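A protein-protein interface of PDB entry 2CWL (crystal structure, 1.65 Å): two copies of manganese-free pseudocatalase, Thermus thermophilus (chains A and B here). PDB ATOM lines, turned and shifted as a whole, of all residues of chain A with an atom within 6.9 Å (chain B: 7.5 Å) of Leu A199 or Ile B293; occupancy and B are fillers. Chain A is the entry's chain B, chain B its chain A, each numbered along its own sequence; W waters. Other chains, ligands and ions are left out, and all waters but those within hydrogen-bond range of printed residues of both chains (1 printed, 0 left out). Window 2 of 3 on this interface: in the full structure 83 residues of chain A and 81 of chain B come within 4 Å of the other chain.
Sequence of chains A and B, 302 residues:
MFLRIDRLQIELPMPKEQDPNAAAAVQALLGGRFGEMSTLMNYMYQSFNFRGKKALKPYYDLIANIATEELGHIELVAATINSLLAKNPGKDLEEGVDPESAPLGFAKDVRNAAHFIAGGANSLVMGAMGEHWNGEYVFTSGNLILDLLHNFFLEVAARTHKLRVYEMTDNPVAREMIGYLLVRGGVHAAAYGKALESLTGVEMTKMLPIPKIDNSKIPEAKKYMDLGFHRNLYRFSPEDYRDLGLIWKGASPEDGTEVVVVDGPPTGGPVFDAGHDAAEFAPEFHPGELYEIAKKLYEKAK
The backbone carbonyl oxygen (O) of Leu B297 sits close to the side-chain carboxylate (OE1) of Glu B299 (2.7 Å).
The side-chain hydroxyl of Tyr A59 sits at hydrogen-bond distance from the side-chain hydroxyl of Ser A198 (2.8 Å).
The side-chain hydroxyl (OG) of Ser A198 lies within hydrogen-bond range of the backbone carbonyl oxygen (O) of Ala A195, 2.7 Å away.
CB of Ala A55 touches CE1 of Tyr B291, 3.4 Å away.
CB of Ala B294 touches O of Ala A55, at 3.4 Å.
Leu B290 touches Leu A56.
Leu A56 touches Tyr B291 (CG to CE1, 3.7 Å).
Ile B293 touches Tyr A59.
Tyr A59 touches Leu B297.
Ser A198 touches Ile B293 (O to CG2, 3.4 Å).
Leu A199 touches Leu B290 (CD2 to CD2, 3.9 Å).
Ile B293 touches Leu A199 (CD1 to O, 3.9 Å).
Of chain B, only Leu B290 (3.9 Å) and Ile B293 (3.9 Å) come within 4 Å of Leu A199.
Of chain A, only Tyr A59, Ser A198 and Leu A199 come within 4 Å of Ile B293.
Of chain B, only Ile B293 (3.4 Å) comes within 4 Å of Ser A198.
Of the printed residues of chain A, Leu B290 touches Leu A56 (3.7 Å) and Leu A199 (3.9 Å).
Of the printed residues of chain B, Ala A55 touches Tyr B291 (3.4 Å) and Ala B294 (3.4 Å).
Val A202 touches none of the printed residues of chain B.
Hydrophobic or aromatic side chains of chain B within 4 Å of the printed part of chain A: Leu B290, Tyr B291, Ile B293, Ala B294 and Leu B297.
Of the 15 printed residues of chain A, 5 touch a printed residue of chain B.
Printed residues of chain A that touch a printed residue of chain B: Ala A55, Leu A56, Tyr A59, Ser A198 and Leu A199.
Hydrophobic or aromatic side chains of chain A that line the printed part of chain B: Ala A55, Leu A56, Tyr A59 and Leu A199.
Among the printed residues, 9 pairs touch across the chains.
Among the printed residues, no Asp or Glu carboxylate lies within 4 Å of a Lys or Arg side-chain nitrogen of the other chain.
No position is printed for both chains.
Water W1 lies within hydrogen-bond range of the backbone carbonyl oxygen (O) of Ala A55 (2.6 Å), the backbone carbonyl oxygen (O) of Tyr B291 (2.9 Å) and the side-chain amino group (NZ) of Lys B295 (2.9 Å).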
ATOM      1  N   ALA A  55     -29.186 -30.206   8.639  1.00  0.00           N
ATOM      2  CA  ALA A  55     -28.922 -29.466   9.873  1.00  0.00           C
ATOM      3  C   ALA A  55     -27.428 -29.227  10.098  1.00  0.00           C
ATOM      4  O   ALA A  55     -27.039 -28.259  10.750  1.00  0.00           O
ATOM      5  CB  ALA A  55     -29.524 -30.207  11.064  1.00  0.00           C
ATOM      6  N   LEU A  56     -26.598 -30.115   9.560  1.00  0.00           N
ATOM      7  CA  LEU A  56     -25.145 -30.003   9.681  1.00  0.00           C
ATOM      8  C   LEU A  56     -24.568 -30.045   8.269  1.00  0.00           C
ATOM      9  O   LEU A  56     -23.504 -30.617   8.028  1.00  0.00           O
ATOM     10  CB  LEU A  56     -24.596 -31.173  10.508  1.00  0.00           C
ATOM     11  CG  LEU A  56     -25.008 -31.205  11.984  1.00  0.00           C
ATOM     12  CD1 LEU A  56     -24.703 -32.569  12.594  1.00  0.00           C
ATOM     13  CD2 LEU A  56     -24.271 -30.104  12.731  1.00  0.00           C
ATOM     14  N   TYR A  59     -20.742 -29.746   7.047  1.00  0.00           N
ATOM     15  CA  TYR A  59     -19.942 -30.923   7.368  1.00  0.00           C
ATOM     16  C   TYR A  59     -20.294 -32.098   6.466  1.00  0.00           C
ATOM     17  O   TYR A  59     -19.430 -32.907   6.122  1.00  0.00           O
ATOM     18  CB  TYR A  59     -20.145 -31.284   8.839  1.00  0.00           C
ATOM     19  CG  TYR A  59     -19.819 -30.127   9.755  1.00  0.00           C
ATOM     20  CD1 TYR A  59     -18.497 -29.794  10.048  1.00  0.00           C
ATOM     21  CD2 TYR A  59     -20.834 -29.325  10.278  1.00  0.00           C
ATOM     22  CE1 TYR A  59     -18.191 -28.684  10.838  1.00  0.00           C
ATOM     23  CE2 TYR A  59     -20.541 -28.215  11.066  1.00  0.00           C
ATOM     24  CZ  TYR A  59     -19.219 -27.900  11.341  1.00  0.00           C
ATOM     25  OH  TYR A  59     -18.927 -26.801  12.113  1.00  0.00           O
ATOM     26  N   LEU A 144     -20.506 -37.343  14.543  1.00  0.00           N
ATOM     27  CA  LEU A 144     -19.722 -36.427  13.718  1.00  0.00           C
ATOM     28  C   LEU A 144     -18.307 -36.119  14.189  1.00  0.00           C
ATOM     29  O   LEU A 144     -17.350 -36.288  13.431  1.00  0.00           O
ATOM     30  CB  LEU A 144     -20.486 -35.113  13.522  1.00  0.00           C
ATOM     31  CG  LEU A 144     -19.791 -34.067  12.641  1.00  0.00           C
ATOM     32  CD1 LEU A 144     -19.501 -34.653  11.266  1.00  0.00           C
ATOM     33  CD2 LEU A 144     -20.681 -32.835  12.517  1.00  0.00           C
ATOM     34  N   ILE A 145     -18.166 -35.659  15.425  1.00  0.00           N
ATOM     35  CA  ILE A 145     -16.846 -35.312  15.934  1.00  0.00           C
ATOM     36  C   ILE A 145     -15.912 -36.518  16.004  1.00  0.00           C
ATOM     37  O   ILE A 145     -14.740 -36.417  15.641  1.00  0.00           O
ATOM     38  CB  ILE A 145     -16.951 -34.626  17.314  1.00  0.00           C
ATOM     39  CG1 ILE A 145     -17.655 -33.275  17.146  1.00  0.00           C
ATOM     40  CG2 ILE A 145     -15.560 -34.428  17.913  1.00  0.00           C
ATOM     41  CD1 ILE A 145     -17.979 -32.562  18.445  1.00  0.00           C
ATOM     42  N   LEU A 148     -14.785 -37.279  12.523  1.00  0.00           N
ATOM     43  CA  LEU A 148     -13.843 -36.277  12.035  1.00  0.00           C
ATOM     44  C   LEU A 148     -12.466 -36.455  12.659  1.00  0.00           C
ATOM     45  O   LEU A 148     -11.449 -36.281  11.985  1.00  0.00           O
ATOM     46  CB  LEU A 148     -14.369 -34.864  12.307  1.00  0.00           C
ATOM     47  CG  LEU A 148     -15.512 -34.406  11.391  1.00  0.00           C
ATOM     48  CD1 LEU A 148     -16.040 -33.070  11.877  1.00  0.00           C
ATOM     49  CD2 LEU A 148     -15.024 -34.299   9.948  1.00  0.00           C
ATOM     50  N   LYS A 194      -9.862 -28.170  10.221  1.00  0.00           N
ATOM     51  CA  LYS A 194     -10.670 -26.958  10.300  1.00  0.00           C
ATOM     52  C   LYS A 194     -12.090 -27.289  10.757  1.00  0.00           C
ATOM     53  O   LYS A 194     -12.711 -26.521  11.498  1.00  0.00           O
ATOM     54  CB  LYS A 194     -10.698 -26.252   8.938  1.00  0.00           C
ATOM     55  CG  LYS A 194      -9.379 -25.574   8.570  1.00  0.00           C
ATOM     56  CD  LYS A 194      -9.416 -24.978   7.166  1.00  0.00           C
ATOM     57  CE  LYS A 194      -8.110 -24.268   6.826  1.00  0.00           C
ATOM     58  NZ  LYS A 194      -7.896 -23.048   7.663  1.00  0.00           N
ATOM     59  N   ALA A 195     -12.603 -28.435  10.318  1.00  0.00           N
ATOM     60  CA  ALA A 195     -13.944 -28.862  10.701  1.00  0.00           C
ATOM     61  C   ALA A 195     -13.983 -29.083  12.208  1.00  0.00           C
ATOM     62  O   ALA A 195     -14.934 -28.686  12.884  1.00  0.00           O
ATOM     63  CB  ALA A 195     -14.318 -30.151   9.969  1.00  0.00           C
ATOM     64  N   LEU A 196     -12.942 -29.723  12.734  1.00  0.00           N
ATOM     65  CA  LEU A 196     -12.858 -29.985  14.165  1.00  0.00           C
ATOM     66  C   LEU A 196     -12.708 -28.686  14.948  1.00  0.00           C
ATOM     67  O   LEU A 196     -13.279 -28.536  16.028  1.00  0.00           O
ATOM     68  CB  LEU A 196     -11.685 -30.925  14.466  1.00  0.00           C
ATOM     69  CG  LEU A 196     -11.932 -32.399  14.120  1.00  0.00           C
ATOM     70  CD1 LEU A 196     -10.627 -33.182  14.175  1.00  0.00           C
ATOM     71  CD2 LEU A 196     -12.949 -32.979  15.090  1.00  0.00           C
ATOM     72  N   GLU A 197     -11.944 -27.745  14.401  1.00  0.00           N
ATOM     73  CA  GLU A 197     -11.739 -26.459  15.062  1.00  0.00           C
ATOM     74  C   GLU A 197     -13.074 -25.726  15.203  1.00  0.00           C
ATOM     75  O   GLU A 197     -13.367 -25.142  16.248  1.00  0.00           O
ATOM     76  CB  GLU A 197     -10.751 -25.596  14.257  1.00  0.00           C
ATOM     77  CG  GLU A 197      -9.393 -26.258  14.032  1.00  0.00           C
ATOM     78  CD  GLU A 197      -8.418 -25.396  13.243  1.00  0.00           C
ATOM     79  OE1 GLU A 197      -8.848 -24.719  12.280  1.00  0.00           O
ATOM     80  OE2 GLU A 197      -7.215 -25.409  13.577  1.00  0.00           O
ATOM     81  N   SER A 198     -13.892 -25.777  14.156  1.00  0.00           N
ATOM     82  CA  SER A 198     -15.187 -25.100  14.171  1.00  0.00           C
ATOM     83  C   SER A 198     -16.193 -25.736  15.123  1.00  0.00           C
ATOM     84  O   SER A 198     -17.066 -25.054  15.659  1.00  0.00           O
ATOM     85  CB  SER A 198     -15.784 -25.059  12.761  1.00  0.00           C
ATOM     86  OG  SER A 198     -16.136 -26.356  12.315  1.00  0.00           O
ATOM     87  N   LEU A 199     -16.065 -27.042  15.338  1.00  0.00           N
ATOM     88  CA  LEU A 199     -16.982 -27.768  16.211  1.00  0.00           C
ATOM     89  C   LEU A 199     -16.523 -27.902  17.659  1.00  0.00           C
ATOM     90  O   LEU A 199     -17.351 -28.075  18.554  1.00  0.00           O
ATOM     91  CB  LEU A 199     -17.225 -29.176  15.657  1.00  0.00           C
ATOM     92  CG  LEU A 199     -17.964 -29.330  14.329  1.00  0.00           C
ATOM     93  CD1 LEU A 199     -17.805 -30.762  13.830  1.00  0.00           C
ATOM     94  CD2 LEU A 199     -19.433 -28.976  14.513  1.00  0.00           C
ATOM     95  N   THR A 200     -15.217 -27.815  17.893  1.00  0.00           N
ATOM     96  CA  THR A 200     -14.681 -27.994  19.240  1.00  0.00           C
ATOM     97  C   THR A 200     -13.849 -26.852  19.806  1.00  0.00           C
ATOM     98  O   THR A 200     -13.684 -26.754  21.020  1.00  0.00           O
ATOM     99  CB  THR A 200     -13.811 -29.258  19.308  1.00  0.00           C
ATOM    100  OG1 THR A 200     -12.593 -29.031  18.587  1.00  0.00           O
ATOM    101  CG2 THR A 200     -14.541 -30.439  18.689  1.00  0.00           C
ATOM    102  N   GLY A 201     -13.303 -26.008  18.939  1.00  0.00           N
ATOM    103  CA  GLY A 201     -12.485 -24.907  19.417  1.00  0.00           C
ATOM    104  C   GLY A 201     -11.029 -25.306  19.587  1.00  0.00           C
ATOM    105  O   GLY A 201     -10.183 -24.472  19.909  1.00  0.00           O
ATOM    106  N   VAL A 202     -10.735 -26.586  19.381  1.00  0.00           N
ATOM    107  CA  VAL A 202      -9.367 -27.084  19.495  1.00  0.00           C
ATOM    108  C   VAL A 202      -8.665 -26.839  18.160  1.00  0.00           C
ATOM    109  O   VAL A 202      -9.173 -27.224  17.107  1.00  0.00           O
ATOM    110  CB  VAL A 202      -9.351 -28.592  19.827  1.00  0.00           C
ATOM    111  CG1 VAL A 202      -7.916 -29.095  19.903  1.00  0.00           C
ATOM    112  CG2 VAL A 202     -10.070 -28.840  21.147  1.00  0.00           C
ATOM    113  N   PRO B 287     -27.552 -32.953  19.652  1.00  0.00           N
ATOM    114  CA  PRO B 287     -26.989 -32.080  18.616  1.00  0.00           C
ATOM    115  C   PRO B 287     -27.399 -30.613  18.606  1.00  0.00           C
ATOM    116  O   PRO B 287     -27.009 -29.873  17.705  1.00  0.00           O
ATOM    117  CB  PRO B 287     -27.392 -32.789  17.331  1.00  0.00           C
ATOM    118  CG  PRO B 287     -28.748 -33.312  17.678  1.00  0.00           C
ATOM    119  CD  PRO B 287     -28.541 -33.879  19.069  1.00  0.00           C
ATOM    120  N   GLY B 288     -28.173 -30.194  19.600  1.00  0.00           N
ATOM    121  CA  GLY B 288     -28.609 -28.809  19.655  1.00  0.00           C
ATOM    122  C   GLY B 288     -27.497 -27.796  19.441  1.00  0.00           C
ATOM    123  O   GLY B 288     -27.604 -26.912  18.586  1.00  0.00           O
ATOM    124  N   GLU B 289     -26.424 -27.922  20.212  1.00  0.00           N
ATOM    125  CA  GLU B 289     -25.303 -27.000  20.103  1.00  0.00           C
ATOM    126  C   GLU B 289     -24.615 -27.058  18.742  1.00  0.00           C
ATOM    127  O   GLU B 289     -24.267 -26.021  18.178  1.00  0.00           O
ATOM    128  CB  GLU B 289     -24.278 -27.274  21.205  1.00  0.00           C
ATOM    129  CG  GLU B 289     -23.081 -26.341  21.165  1.00  0.00           C
ATOM    130  CD  GLU B 289     -22.121 -26.574  22.313  1.00  0.00           C
ATOM    131  OE1 GLU B 289     -21.594 -27.701  22.432  1.00  0.00           O
ATOM    132  OE2 GLU B 289     -21.895 -25.628  23.096  1.00  0.00           O
ATOM    133  N   LEU B 290     -24.407 -28.261  18.216  1.00  0.00           N
ATOM    134  CA  LEU B 290     -23.754 -28.385  16.920  1.00  0.00           C
ATOM    135  C   LEU B 290     -24.600 -27.756  15.817  1.00  0.00           C
ATOM    136  O   LEU B 290     -24.066 -27.155  14.886  1.00  0.00           O
ATOM    137  CB  LEU B 290     -23.468 -29.856  16.595  1.00  0.00           C
ATOM    138  CG  LEU B 290     -22.532 -30.586  17.566  1.00  0.00           C
ATOM    139  CD1 LEU B 290     -22.117 -31.909  16.945  1.00  0.00           C
ATOM    140  CD2 LEU B 290     -21.300 -29.739  17.862  1.00  0.00           C
ATOM    141  N   TYR B 291     -25.920 -27.883  15.923  1.00  0.00           N
ATOM    142  CA  TYR B 291     -26.806 -27.297  14.921  1.00  0.00           C
ATOM    143  C   TYR B 291     -26.679 -25.775  14.941  1.00  0.00           C
ATOM    144  O   TYR B 291     -26.748 -25.125  13.898  1.00  0.00           O
ATOM    145  CB  TYR B 291     -28.267 -27.691  15.170  1.00  0.00           C
ATOM    146  CG  TYR B 291     -28.588 -29.160  14.961  1.00  0.00           C
ATOM    147  CD1 TYR B 291     -27.765 -29.979  14.182  1.00  0.00           C
ATOM    148  CD2 TYR B 291     -29.743 -29.720  15.510  1.00  0.00           C
ATOM    149  CE1 TYR B 291     -28.088 -31.323  13.958  1.00  0.00           C
ATOM    150  CE2 TYR B 291     -30.074 -31.058  15.290  1.00  0.00           C
ATOM    151  CZ  TYR B 291     -29.245 -31.851  14.515  1.00  0.00           C
ATOM    152  OH  TYR B 291     -29.583 -33.166  14.295  1.00  0.00           O
ATOM    153  N   GLU B 292     -26.499 -25.209  16.132  1.00  0.00           N
ATOM    154  CA  GLU B 292     -26.349 -23.764  16.263  1.00  0.00           C
ATOM    155  C   GLU B 292     -25.027 -23.327  15.649  1.00  0.00           C
ATOM    156  O   GLU B 292     -24.949 -22.287  14.999  1.00  0.00           O
ATOM    157  CB  GLU B 292     -26.403 -23.346  17.735  1.00  0.00           C
ATOM    158  CG  GLU B 292     -27.790 -23.427  18.345  1.00  0.00           C
ATOM    159  CD  GLU B 292     -28.803 -22.599  17.578  1.00  0.00           C
ATOM    160  OE1 GLU B 292     -28.554 -21.390  17.376  1.00  0.00           O
ATOM    161  OE2 GLU B 292     -29.849 -23.156  17.177  1.00  0.00           O
ATOM    162  N   ILE B 293     -23.986 -24.127  15.862  1.00  0.00           N
ATOM    163  CA  ILE B 293     -22.673 -23.826  15.305  1.00  0.00           C
ATOM    164  C   ILE B 293     -22.765 -23.828  13.784  1.00  0.00           C
ATOM    165  O   ILE B 293     -22.223 -22.945  13.120  1.00  0.00           O
ATOM    166  CB  ILE B 293     -21.624 -24.867  15.758  1.00  0.00           C
ATOM    167  CG1 ILE B 293     -21.343 -24.696  17.254  1.00  0.00           C
ATOM    168  CG2 ILE B 293     -20.345 -24.717  14.942  1.00  0.00           C
ATOM    169  CD1 ILE B 293     -20.393 -25.730  17.830  1.00  0.00           C
ATOM    170  N   ALA B 294     -23.460 -24.821  13.237  1.00  0.00           N
ATOM    171  CA  ALA B 294     -23.626 -24.928  11.794  1.00  0.00           C
ATOM    172  C   ALA B 294     -24.357 -23.701  11.258  1.00  0.00           C
ATOM    173  O   ALA B 294     -23.940 -23.104  10.269  1.00  0.00           O
ATOM    174  CB  ALA B 294     -24.404 -26.195  11.445  1.00  0.00           C
ATOM    175  N   LYS B 295     -25.451 -23.331  11.917  1.00  0.00           N
ATOM    176  CA  LYS B 295     -26.232 -22.170  11.503  1.00  0.00           C
ATOM    177  C   LYS B 295     -25.369 -20.912  11.470  1.00  0.00           C
ATOM    178  O   LYS B 295     -25.457 -20.113  10.537  1.00  0.00           O
ATOM    179  CB  LYS B 295     -27.409 -21.951  12.457  1.00  0.00           C
ATOM    180  CG  LYS B 295     -28.489 -23.019  12.386  1.00  0.00           C
ATOM    181  CD  LYS B 295     -29.612 -22.727  13.372  1.00  0.00           C
ATOM    182  CE  LYS B 295     -30.735 -23.747  13.258  1.00  0.00           C
ATOM    183  NZ  LYS B 295     -30.269 -25.132  13.542  1.00  0.00           N
ATOM    184  N   LYS B 296     -24.533 -20.742  12.491  1.00  0.00           N
ATOM    185  CA  LYS B 296     -23.663 -19.575  12.577  1.00  0.00           C
ATOM    186  C   LYS B 296     -22.611 -19.519  11.471  1.00  0.00           C
ATOM    187  O   LYS B 296     -22.119 -18.443  11.135  1.00  0.00           O
ATOM    188  CB  LYS B 296     -22.980 -19.527  13.947  1.00  0.00           C
ATOM    189  CG  LYS B 296     -23.942 -19.293  15.105  1.00  0.00           C
ATOM    190  CD  LYS B 296     -23.208 -19.222  16.435  1.00  0.00           C
ATOM    191  CE  LYS B 296     -24.176 -19.036  17.598  1.00  0.00           C
ATOM    192  NZ  LYS B 296     -24.961 -17.775  17.480  1.00  0.00           N
ATOM    193  N   LEU B 297     -22.265 -20.671  10.904  1.00  0.00           N
ATOM    194  CA  LEU B 297     -21.274 -20.705   9.831  1.00  0.00           C
ATOM    195  C   LEU B 297     -21.754 -19.915   8.616  1.00  0.00           C
ATOM    196  O   LEU B 297     -20.954 -19.325   7.891  1.00  0.00           O
ATOM    197  CB  LEU B 297     -20.977 -22.150   9.416  1.00  0.00           C
ATOM    198  CG  LEU B 297     -20.256 -23.031  10.439  1.00  0.00           C
ATOM    199  CD1 LEU B 297     -20.032 -24.413   9.843  1.00  0.00           C
ATOM    200  CD2 LEU B 297     -18.924 -22.400  10.824  1.00  0.00           C
ATOM    201  N   TYR B 298     -23.065 -19.914   8.399  1.00  0.00           N
ATOM    202  CA  TYR B 298     -23.663 -19.196   7.280  1.00  0.00           C
ATOM    203  C   TYR B 298     -23.727 -17.703   7.587  1.00  0.00           C
ATOM    204  O   TYR B 298     -24.197 -16.913   6.767  1.00  0.00           O
ATOM    205  CB  TYR B 298     -25.076 -19.724   7.018  1.00  0.00           C
ATOM    206  CG  TYR B 298     -25.120 -21.130   6.458  1.00  0.00           C
ATOM    207  CD1 TYR B 298     -25.063 -21.357   5.083  1.00  0.00           C
ATOM    208  CD2 TYR B 298     -25.200 -22.235   7.305  1.00  0.00           C
ATOM    209  CE1 TYR B 298     -25.083 -22.651   4.563  1.00  0.00           C
ATOM    210  CE2 TYR B 298     -25.218 -23.533   6.796  1.00  0.00           C
ATOM    211  CZ  TYR B 298     -25.159 -23.732   5.426  1.00  0.00           C
ATOM    212  OH  TYR B 298     -25.166 -25.013   4.921  1.00  0.00           O
ATOM    213  N   GLU B 299     -23.246 -17.330   8.771  1.00  0.00           N
ATOM    214  CA  GLU B 299     -23.256 -15.942   9.223  1.00  0.00           C
ATOM    215  C   GLU B 299     -24.686 -15.475   9.467  1.00  0.00           C
ATOM    216  O   GLU B 299     -25.024 -15.222  10.642  1.00  0.00           O
ATOM    217  CB  GLU B 299     -22.582 -15.024   8.197  1.00  0.00           C
ATOM    218  CG  GLU B 299     -21.069 -14.942   8.322  1.00  0.00           C
ATOM    219  CD  GLU B 299     -20.384 -16.277   8.120  1.00  0.00           C
ATOM    220  OE1 GLU B 299     -20.488 -16.838   7.008  1.00  0.00           O
ATOM    221  OE2 GLU B 299     -19.742 -16.765   9.073  1.00  0.00           O
HETATM  222  O   HOH W   1     -28.304 -26.234  11.767  1.00  0.00           O
